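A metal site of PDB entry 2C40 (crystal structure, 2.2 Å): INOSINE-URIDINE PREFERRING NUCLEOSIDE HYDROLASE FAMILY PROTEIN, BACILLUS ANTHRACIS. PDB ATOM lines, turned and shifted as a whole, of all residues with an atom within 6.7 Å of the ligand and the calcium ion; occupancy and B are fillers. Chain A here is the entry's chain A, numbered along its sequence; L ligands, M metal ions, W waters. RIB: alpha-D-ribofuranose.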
ATOM      1  N   HIS A   8       2.302 -23.174   4.353  1.00  0.00           N
ATOM      2  CA  HIS A   8       1.677 -23.637   3.097  1.00  0.00           C
ATOM      3  C   HIS A   8       1.523 -22.511   2.119  1.00  0.00           C
ATOM      4  O   HIS A   8       1.572 -21.360   2.515  1.00  0.00           O
ATOM      5  CB  HIS A   8       0.328 -24.341   3.349  1.00  0.00           C
ATOM      6  CG  HIS A   8      -0.827 -23.437   3.743  1.00  0.00           C
ATOM      7  ND1 HIS A   8      -1.618 -22.777   2.833  1.00  0.00           N
ATOM      8  CD2 HIS A   8      -1.375 -23.191   4.965  1.00  0.00           C
ATOM      9  CE1 HIS A   8      -2.559 -22.114   3.474  1.00  0.00           C
ATOM     10  NE2 HIS A   8      -2.442 -22.353   4.779  1.00  0.00           N
ATOM     11  N   ASP A   9       1.314 -22.831   0.840  1.00  0.00           N
ATOM     12  CA  ASP A   9       1.087 -21.762  -0.138  1.00  0.00           C
ATOM     13  C   ASP A   9      -0.290 -21.759  -0.801  1.00  0.00           C
ATOM     14  O   ASP A   9      -0.413 -21.389  -1.929  1.00  0.00           O
ATOM     15  CB  ASP A   9       2.199 -21.691  -1.182  1.00  0.00           C
ATOM     16  CG  ASP A   9       2.253 -22.872  -2.086  1.00  0.00           C
ATOM     17  OD1 ASP A   9       2.916 -22.741  -3.135  1.00  0.00           O
ATOM     18  OD2 ASP A   9       1.665 -23.924  -1.759  1.00  0.00           O
ATOM     19  N   GLY A  10      -1.294 -22.221  -0.073  1.00  0.00           N
ATOM     20  CA  GLY A  10      -2.699 -21.924  -0.359  1.00  0.00           C
ATOM     21  C   GLY A  10      -3.288 -22.437  -1.649  1.00  0.00           C
ATOM     22  O   GLY A  10      -4.310 -21.931  -2.054  1.00  0.00           O
ATOM     23  N   GLY A  11      -2.652 -23.405  -2.311  1.00  0.00           N
ATOM     24  CA  GLY A  11      -3.340 -24.207  -3.349  1.00  0.00           C
ATOM     25  C   GLY A  11      -4.463 -25.010  -2.693  1.00  0.00           C
ATOM     26  O   GLY A  11      -4.620 -25.022  -1.472  1.00  0.00           O
ATOM     27  N   VAL A  12      -5.283 -25.646  -3.506  1.00  0.00           N
ATOM     28  CA  VAL A  12      -6.375 -26.504  -3.004  1.00  0.00           C
ATOM     29  C   VAL A  12      -5.859 -27.565  -2.050  1.00  0.00           C
ATOM     30  O   VAL A  12      -6.478 -27.818  -1.010  1.00  0.00           O
ATOM     31  CB  VAL A  12      -7.163 -27.124  -4.169  1.00  0.00           C
ATOM     32  CG1 VAL A  12      -7.983 -28.352  -3.719  1.00  0.00           C
ATOM     33  CG2 VAL A  12      -8.071 -26.085  -4.733  1.00  0.00           C
ATOM     34  N   ASP A  13      -4.740 -28.200  -2.378  1.00  0.00           N
ATOM     35  CA  ASP A  13      -4.282 -29.314  -1.525  1.00  0.00           C
ATOM     36  C   ASP A  13      -3.564 -28.846  -0.234  1.00  0.00           C
ATOM     37  O   ASP A  13      -3.516 -29.606   0.728  1.00  0.00           O
ATOM     38  CB  ASP A  13      -3.507 -30.413  -2.310  1.00  0.00           C
ATOM     39  CG  ASP A  13      -2.225 -29.929  -2.911  1.00  0.00           C
ATOM     40  OD1 ASP A  13      -1.871 -28.756  -2.639  1.00  0.00           O
ATOM     41  OD2 ASP A  13      -1.564 -30.725  -3.645  1.00  0.00           O
ATOM     42  N   ASP A  14      -3.061 -27.606  -0.226  1.00  0.00           N
ATOM     43  CA  ASP A  14      -2.570 -26.955   0.995  1.00  0.00           C
ATOM     44  C   ASP A  14      -3.713 -26.741   1.975  1.00  0.00           C
ATOM     45  O   ASP A  14      -3.590 -26.954   3.161  1.00  0.00           O
ATOM     46  CB  ASP A  14      -1.957 -25.585   0.683  1.00  0.00           C
ATOM     47  CG  ASP A  14      -0.691 -25.671  -0.146  1.00  0.00           C
ATOM     48  OD1 ASP A  14       0.413 -25.878   0.431  1.00  0.00           O
ATOM     49  OD2 ASP A  14      -0.770 -25.558  -1.389  1.00  0.00           O
ATOM     50  N   ASP A  38       1.887 -20.338  -4.637  1.00  0.00           N
ATOM     51  CA  ASP A  38       0.800 -20.830  -5.490  1.00  0.00           C
ATOM     52  C   ASP A  38      -0.569 -20.289  -5.064  1.00  0.00           C
ATOM     53  O   ASP A  38      -1.572 -20.995  -5.090  1.00  0.00           O
ATOM     54  CB  ASP A  38       0.807 -22.334  -5.486  1.00  0.00           C
ATOM     55  CG  ASP A  38       0.033 -22.927  -6.610  1.00  0.00           C
ATOM     56  OD1 ASP A  38      -0.280 -24.113  -6.454  1.00  0.00           O
ATOM     57  OD2 ASP A  38      -0.280 -22.234  -7.592  1.00  0.00           O
ATOM     58  N   PHE A  73       4.637 -18.543  -9.495  1.00  0.00           N
ATOM     59  CA  PHE A  73       3.743 -19.568 -10.064  1.00  0.00           C
ATOM     60  C   PHE A  73       2.840 -18.985 -11.142  1.00  0.00           C
ATOM     61  O   PHE A  73       2.677 -17.762 -11.213  1.00  0.00           O
ATOM     62  CB  PHE A  73       2.862 -20.173  -8.968  1.00  0.00           C
ATOM     63  CG  PHE A  73       3.510 -21.274  -8.143  1.00  0.00           C
ATOM     64  CD1 PHE A  73       4.341 -20.973  -7.046  1.00  0.00           C
ATOM     65  CD2 PHE A  73       3.213 -22.582  -8.374  1.00  0.00           C
ATOM     66  CE1 PHE A  73       4.911 -21.926  -6.300  1.00  0.00           C
ATOM     67  CE2 PHE A  73       3.763 -23.597  -7.581  1.00  0.00           C
ATOM     68  CZ  PHE A  73       4.641 -23.274  -6.565  1.00  0.00           C
ATOM     69  N   TRP A  77      -3.181 -21.011 -11.597  1.00  0.00           N
ATOM     70  CA  TRP A  77      -3.066 -21.875 -10.404  1.00  0.00           C
ATOM     71  C   TRP A  77      -3.276 -21.066  -9.119  1.00  0.00           C
ATOM     72  O   TRP A  77      -3.957 -21.491  -8.185  1.00  0.00           O
ATOM     73  CB  TRP A  77      -1.656 -22.471 -10.363  1.00  0.00           C
ATOM     74  CG  TRP A  77      -1.321 -23.404 -11.479  1.00  0.00           C
ATOM     75  CD1 TRP A  77      -2.022 -23.586 -12.667  1.00  0.00           C
ATOM     76  CD2 TRP A  77      -0.168 -24.254 -11.549  1.00  0.00           C
ATOM     77  NE1 TRP A  77      -1.359 -24.521 -13.438  1.00  0.00           N
ATOM     78  CE2 TRP A  77      -0.231 -24.954 -12.774  1.00  0.00           C
ATOM     79  CE3 TRP A  77       0.909 -24.504 -10.683  1.00  0.00           C
ATOM     80  CZ2 TRP A  77       0.743 -25.870 -13.159  1.00  0.00           C
ATOM     81  CZ3 TRP A  77       1.863 -25.420 -11.057  1.00  0.00           C
ATOM     82  CH2 TRP A  77       1.792 -26.089 -12.280  1.00  0.00           C
ATOM     83  N   THR A 125       4.461 -27.207   2.649  1.00  0.00           N
ATOM     84  CA  THR A 125       3.829 -27.652   1.455  1.00  0.00           C
ATOM     85  C   THR A 125       3.843 -26.626   0.303  1.00  0.00           C
ATOM     86  O   THR A 125       3.353 -26.943  -0.771  1.00  0.00           O
ATOM     87  CB  THR A 125       2.406 -28.203   1.708  1.00  0.00           C
ATOM     88  OG1 THR A 125       1.513 -27.196   2.234  1.00  0.00           O
ATOM     89  CG2 THR A 125       2.475 -29.383   2.638  1.00  0.00           C
ATOM     90  N   GLY A 126       4.483 -25.481   0.509  1.00  0.00           N
ATOM     91  CA  GLY A 126       4.898 -24.568  -0.528  1.00  0.00           C
ATOM     92  C   GLY A 126       6.433 -24.484  -0.560  1.00  0.00           C
ATOM     93  O   GLY A 126       7.128 -25.334  -0.005  1.00  0.00           O
ATOM     94  N   PRO A 127       6.994 -23.445  -1.227  1.00  0.00           N
ATOM     95  CA  PRO A 127       8.420 -23.127  -1.231  1.00  0.00           C
ATOM     96  C   PRO A 127       9.040 -22.982   0.169  1.00  0.00           C
ATOM     97  O   PRO A 127       8.294 -22.814   1.126  1.00  0.00           O
ATOM     98  CB  PRO A 127       8.421 -21.771  -1.925  1.00  0.00           C
ATOM     99  CG  PRO A 127       7.269 -21.816  -2.843  1.00  0.00           C
ATOM    100  CD  PRO A 127       6.231 -22.481  -2.023  1.00  0.00           C
ATOM    101  N   MET A 151       7.191 -31.058   0.806  1.00  0.00           N
ATOM    102  CA  MET A 151       6.809 -31.326  -0.552  1.00  0.00           C
ATOM    103  C   MET A 151       7.707 -30.520  -1.478  1.00  0.00           C
ATOM    104  O   MET A 151       7.580 -29.295  -1.620  1.00  0.00           O
ATOM    105  CB  MET A 151       5.337 -30.988  -0.792  1.00  0.00           C
ATOM    106  CG  MET A 151       4.750 -31.661  -2.100  1.00  0.00           C
ATOM    107  SD  MET A 151       5.298 -30.967  -3.697  1.00  0.00           S
ATOM    108  CE  MET A 151       5.856 -32.416  -4.519  1.00  0.00           C
ATOM    109  N   GLY A 152       8.607 -31.200  -2.128  1.00  0.00           N
ATOM    110  CA  GLY A 152       9.496 -30.541  -3.091  1.00  0.00           C
ATOM    111  C   GLY A 152      10.370 -31.548  -3.797  1.00  0.00           C
ATOM    112  O   GLY A 152      10.534 -32.709  -3.362  1.00  0.00           O
ATOM    113  N   ASN A 160       7.790 -30.622 -13.166  1.00  0.00           N
ATOM    114  CA  ASN A 160       6.451 -30.074 -13.533  1.00  0.00           C
ATOM    115  C   ASN A 160       6.530 -28.582 -13.803  1.00  0.00           C
ATOM    116  O   ASN A 160       5.486 -27.894 -14.007  1.00  0.00           O
ATOM    117  CB  ASN A 160       5.455 -30.324 -12.424  1.00  0.00           C
ATOM    118  CG  ASN A 160       5.862 -29.654 -11.107  1.00  0.00           C
ATOM    119  OD1 ASN A 160       7.011 -29.242 -10.943  1.00  0.00           O
ATOM    120  ND2 ASN A 160       4.932 -29.536 -10.193  1.00  0.00           N
ATOM    121  N   VAL A 161       7.769 -28.092 -13.880  1.00  0.00           N
ATOM    122  CA  VAL A 161       8.046 -26.711 -14.295  1.00  0.00           C
ATOM    123  C   VAL A 161       8.300 -26.659 -15.819  1.00  0.00           C
ATOM    124  O   VAL A 161       9.273 -27.229 -16.317  1.00  0.00           O
ATOM    125  CB  VAL A 161       9.283 -26.122 -13.515  1.00  0.00           C
ATOM    126  CG1 VAL A 161       9.590 -24.732 -13.941  1.00  0.00           C
ATOM    127  CG2 VAL A 161       9.001 -26.060 -12.044  1.00  0.00           C
ATOM    128  N   GLU A 171      11.115 -29.193  -9.911  1.00  0.00           N
ATOM    129  CA  GLU A 171       9.778 -29.230  -9.365  1.00  0.00           C
ATOM    130  C   GLU A 171       9.474 -27.798  -8.857  1.00  0.00           C
ATOM    131  O   GLU A 171      10.395 -27.053  -8.514  1.00  0.00           O
ATOM    132  CB  GLU A 171       9.751 -30.283  -8.274  1.00  0.00           C
ATOM    133  CG  GLU A 171       8.561 -30.312  -7.414  1.00  0.00           C
ATOM    134  CD  GLU A 171       8.570 -29.241  -6.358  1.00  0.00           C
ATOM    135  OE1 GLU A 171       7.440 -28.844  -6.062  1.00  0.00           O
ATOM    136  OE2 GLU A 171       9.668 -28.793  -5.849  1.00  0.00           O
ATOM    137  N   TRP A 172       8.187 -27.420  -8.854  1.00  0.00           N
ATOM    138  CA  TRP A 172       7.757 -26.041  -8.593  1.00  0.00           C
ATOM    139  C   TRP A 172       8.113 -25.420  -7.246  1.00  0.00           C
ATOM    140  O   TRP A 172       8.477 -24.237  -7.175  1.00  0.00           O
ATOM    141  CB  TRP A 172       6.227 -25.869  -8.870  1.00  0.00           C
ATOM    142  CG  TRP A 172       5.954 -25.232 -10.197  1.00  0.00           C
ATOM    143  CD1 TRP A 172       5.460 -25.827 -11.326  1.00  0.00           C
ATOM    144  CD2 TRP A 172       6.262 -23.885 -10.566  1.00  0.00           C
ATOM    145  NE1 TRP A 172       5.395 -24.923 -12.350  1.00  0.00           N
ATOM    146  CE2 TRP A 172       5.889 -23.724 -11.903  1.00  0.00           C
ATOM    147  CE3 TRP A 172       6.776 -22.790  -9.855  1.00  0.00           C
ATOM    148  CZ2 TRP A 172       6.065 -22.517 -12.583  1.00  0.00           C
ATOM    149  CZ3 TRP A 172       6.923 -21.592 -10.503  1.00  0.00           C
ATOM    150  CH2 TRP A 172       6.568 -21.461 -11.863  1.00  0.00           C
ATOM    151  N   ASN A 173       7.890 -26.135  -6.138  1.00  0.00           N
ATOM    152  CA  ASN A 173       8.243 -25.562  -4.824  1.00  0.00           C
ATOM    153  C   ASN A 173       9.736 -25.223  -4.710  1.00  0.00           C
ATOM    154  O   ASN A 173      10.090 -24.216  -4.096  1.00  0.00           O
ATOM    155  CB  ASN A 173       7.774 -26.459  -3.663  1.00  0.00           C
ATOM    156  CG  ASN A 173       6.230 -26.449  -3.485  1.00  0.00           C
ATOM    157  OD1 ASN A 173       5.552 -25.544  -3.968  1.00  0.00           O
ATOM    158  ND2 ASN A 173       5.705 -27.433  -2.757  1.00  0.00           N
ATOM    159  N   SER A 174      10.602 -26.044  -5.316  1.00  0.00           N
ATOM    160  CA  SER A 174      12.023 -25.752  -5.402  1.00  0.00           C
ATOM    161  C   SER A 174      12.302 -24.606  -6.370  1.00  0.00           C
ATOM    162  O   SER A 174      13.010 -23.661  -6.037  1.00  0.00           O
ATOM    163  CB  SER A 174      12.841 -26.959  -5.864  1.00  0.00           C
ATOM    164  OG  SER A 174      12.435 -28.135  -5.201  1.00  0.00           O
ATOM    165  N   LEU A 196       7.785 -35.215  -6.440  1.00  0.00           N
ATOM    166  CA  LEU A 196       6.787 -35.543  -7.439  1.00  0.00           C
ATOM    167  C   LEU A 196       6.506 -37.047  -7.581  1.00  0.00           C
ATOM    168  O   LEU A 196       5.322 -37.430  -7.692  1.00  0.00           O
ATOM    169  CB  LEU A 196       7.144 -34.933  -8.790  1.00  0.00           C
ATOM    170  CG  LEU A 196       7.186 -33.389  -8.834  1.00  0.00           C
ATOM    171  CD1 LEU A 196       7.738 -32.908 -10.191  1.00  0.00           C
ATOM    172  CD2 LEU A 196       5.814 -32.740  -8.563  1.00  0.00           C
ATOM    173  N   TYR A 243      -4.633 -36.728 -11.234  1.00  0.00           N
ATOM    174  CA  TYR A 243      -4.122 -35.660 -10.353  1.00  0.00           C
ATOM    175  C   TYR A 243      -3.569 -36.269  -9.048  1.00  0.00           C
ATOM    176  O   TYR A 243      -4.129 -37.183  -8.484  1.00  0.00           O
ATOM    177  CB  TYR A 243      -5.271 -34.679 -10.106  1.00  0.00           C
ATOM    178  CG  TYR A 243      -5.103 -33.593  -9.088  1.00  0.00           C
ATOM    179  CD1 TYR A 243      -5.094 -33.880  -7.709  1.00  0.00           C
ATOM    180  CD2 TYR A 243      -5.057 -32.263  -9.484  1.00  0.00           C
ATOM    181  CE1 TYR A 243      -4.972 -32.869  -6.762  1.00  0.00           C
ATOM    182  CE2 TYR A 243      -4.926 -31.232  -8.547  1.00  0.00           C
ATOM    183  CZ  TYR A 243      -4.898 -31.528  -7.199  1.00  0.00           C
ATOM    184  OH  TYR A 243      -4.808 -30.483  -6.299  1.00  0.00           O
ATOM    185  N   TRP A 246      -0.106 -34.134  -3.698  1.00  0.00           N
ATOM    186  CA  TRP A 246       1.247 -34.060  -3.170  1.00  0.00           C
ATOM    187  C   TRP A 246       1.342 -33.510  -1.774  1.00  0.00           C
ATOM    188  O   TRP A 246       2.002 -34.090  -0.944  1.00  0.00           O
ATOM    189  CB  TRP A 246       2.082 -33.163  -4.039  1.00  0.00           C
ATOM    190  CG  TRP A 246       2.413 -33.779  -5.279  1.00  0.00           C
ATOM    191  CD1 TRP A 246       3.303 -34.761  -5.483  1.00  0.00           C
ATOM    192  CD2 TRP A 246       1.860 -33.443  -6.548  1.00  0.00           C
ATOM    193  NE1 TRP A 246       3.330 -35.099  -6.815  1.00  0.00           N
ATOM    194  CE2 TRP A 246       2.457 -34.296  -7.493  1.00  0.00           C
ATOM    195  CE3 TRP A 246       0.874 -32.548  -6.955  1.00  0.00           C
ATOM    196  CZ2 TRP A 246       2.147 -34.257  -8.859  1.00  0.00           C
ATOM    197  CZ3 TRP A 246       0.554 -32.518  -8.322  1.00  0.00           C
ATOM    198  CH2 TRP A 246       1.203 -33.364  -9.248  1.00  0.00           C
ATOM    199  N   ASP A 247       0.659 -32.408  -1.544  1.00  0.00           N
ATOM    200  CA  ASP A 247       0.673 -31.760  -0.239  1.00  0.00           C
ATOM    201  C   ASP A 247      -0.086 -32.560   0.851  1.00  0.00           C
ATOM    202  O   ASP A 247       0.351 -32.635   1.998  1.00  0.00           O
ATOM    203  CB  ASP A 247       0.104 -30.356  -0.361  1.00  0.00           C
ATOM    204  CG  ASP A 247       0.900 -29.511  -1.360  1.00  0.00           C
ATOM    205  OD1 ASP A 247       2.047 -29.906  -1.718  1.00  0.00           O
ATOM    206  OD2 ASP A 247       0.416 -28.420  -1.723  1.00  0.00           O
HETATM  207  O5  RIB L   1       4.999 -28.741  -7.419  1.00  0.00           O
HETATM  208  C5  RIB L   1       3.824 -29.204  -6.703  1.00  0.00           C
HETATM  209  C4  RIB L   1       3.294 -28.028  -5.875  1.00  0.00           C
HETATM  210  O4  RIB L   1       2.815 -27.049  -6.825  1.00  0.00           O
HETATM  211  C3  RIB L   1       2.163 -28.297  -4.861  1.00  0.00           C
HETATM  212  O3  RIB L   1       2.720 -28.146  -3.507  1.00  0.00           O
HETATM  213  C2  RIB L   1       0.960 -27.322  -5.263  1.00  0.00           C
HETATM  214  O2  RIB L   1       0.226 -26.455  -4.281  1.00  0.00           O
HETATM  215  C1  RIB L   1       1.560 -26.453  -6.392  1.00  0.00           C
HETATM  216 CA    CA M   1       1.406 -26.217  -2.192  1.00  0.00          CA
HETATM  217  O   HOH W   1       2.975 -25.245  -3.835  1.00  0.00           O
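OG of Ser 174 lies within hydrogen-bond range of OE2 of Glu 171 (2.9 Å). The side-chain amide nitrogen (ND2) of Asn 173 sits close to the backbone carbonyl oxygen (O) of Thr 125, 3.1 Å away. The backbone NH (N) of Gly 11 lies close to the side-chain carboxylate (OD2) of Asp 14 (3.0 Å). N of Asp 38 lies within hydrogen-bond range of OD1 of Asp 9, 3.0 Å away. The backbone NH of Asp 247 is in hydrogen-bond range of the side-chain carboxylate of Asp 13, at 3.5 Å. N of Trp 172 sits at hydrogen-bond distance from OD1 of Asn 160, at 3.0 Å. The side-chain amide nitrogen of Asn 173 lies within hydrogen-bond range of the backbone carbonyl oxygen of Met 151 (2.9 Å). The side-chain carboxylate (OE1) of Glu 171 is in hydrogen-bond range of the backbone NH (N) of Asn 173, 2.7 Å away.
OD1 of Asp 13 touches O2 of the ligand, at 3.5 Å. Phe 73 touches the ligand. Met 151 touches the ligand (SD to C5, 3.8 Å). CB of Trp 172 touches O5 of the ligand (3.4 Å). Hydrophobic or aromatic side chains that line the ligand: Phe 73, Met 151 and Trp 172. Within 4 Å of the ligand: Asp 9, Asp 13, Asp 14, Asp 38, Phe 73, Thr 125, Met 151, Asn 160, Glu 171, Trp 172, Asn 173 and Asp 247. Along chain A the residues within 4 Å of the ligand span positions 9 to 247. The nearest printed residue that does not touch the ligand is Leu 196 (4.2 Å).
The side-chain amide nitrogen (ND2) of Asn 173 lies close to an oxygen (O3) of the ligand, at 3.2 Å. OD1 of Asp 38 sits close to O2 of the ligand, 3.2 Å away. ND2 of Asn 160 lies within hydrogen-bond range of O5 of the ligand (2.9 Å). O5 of the ligand lies within hydrogen-bond range of OE1 of Glu 171, at 2.8 Å.
The calcium ion is bound by the side-chain carboxylate (OD2) of Asp 9 (2.3 Å). O2 of the ligand is bound to the calcium ion (2.4 Å). OD2 of Asp 14 is bound to the calcium ion. OD2 of Asp 247 binds the calcium ion (2.5 Å). Water W1 is bound to the calcium ion (2.5 Å). The calcium ion is bound by the backbone carbonyl oxygen (O) of Thr 125 (2.5 Å). O3 of the ligand is bound to the calcium ion (2.7 Å). The side-chain carboxylate (OD1) of Asp 14 is bound to the calcium ion. The calcium ion has eight donor atoms within binding distance.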
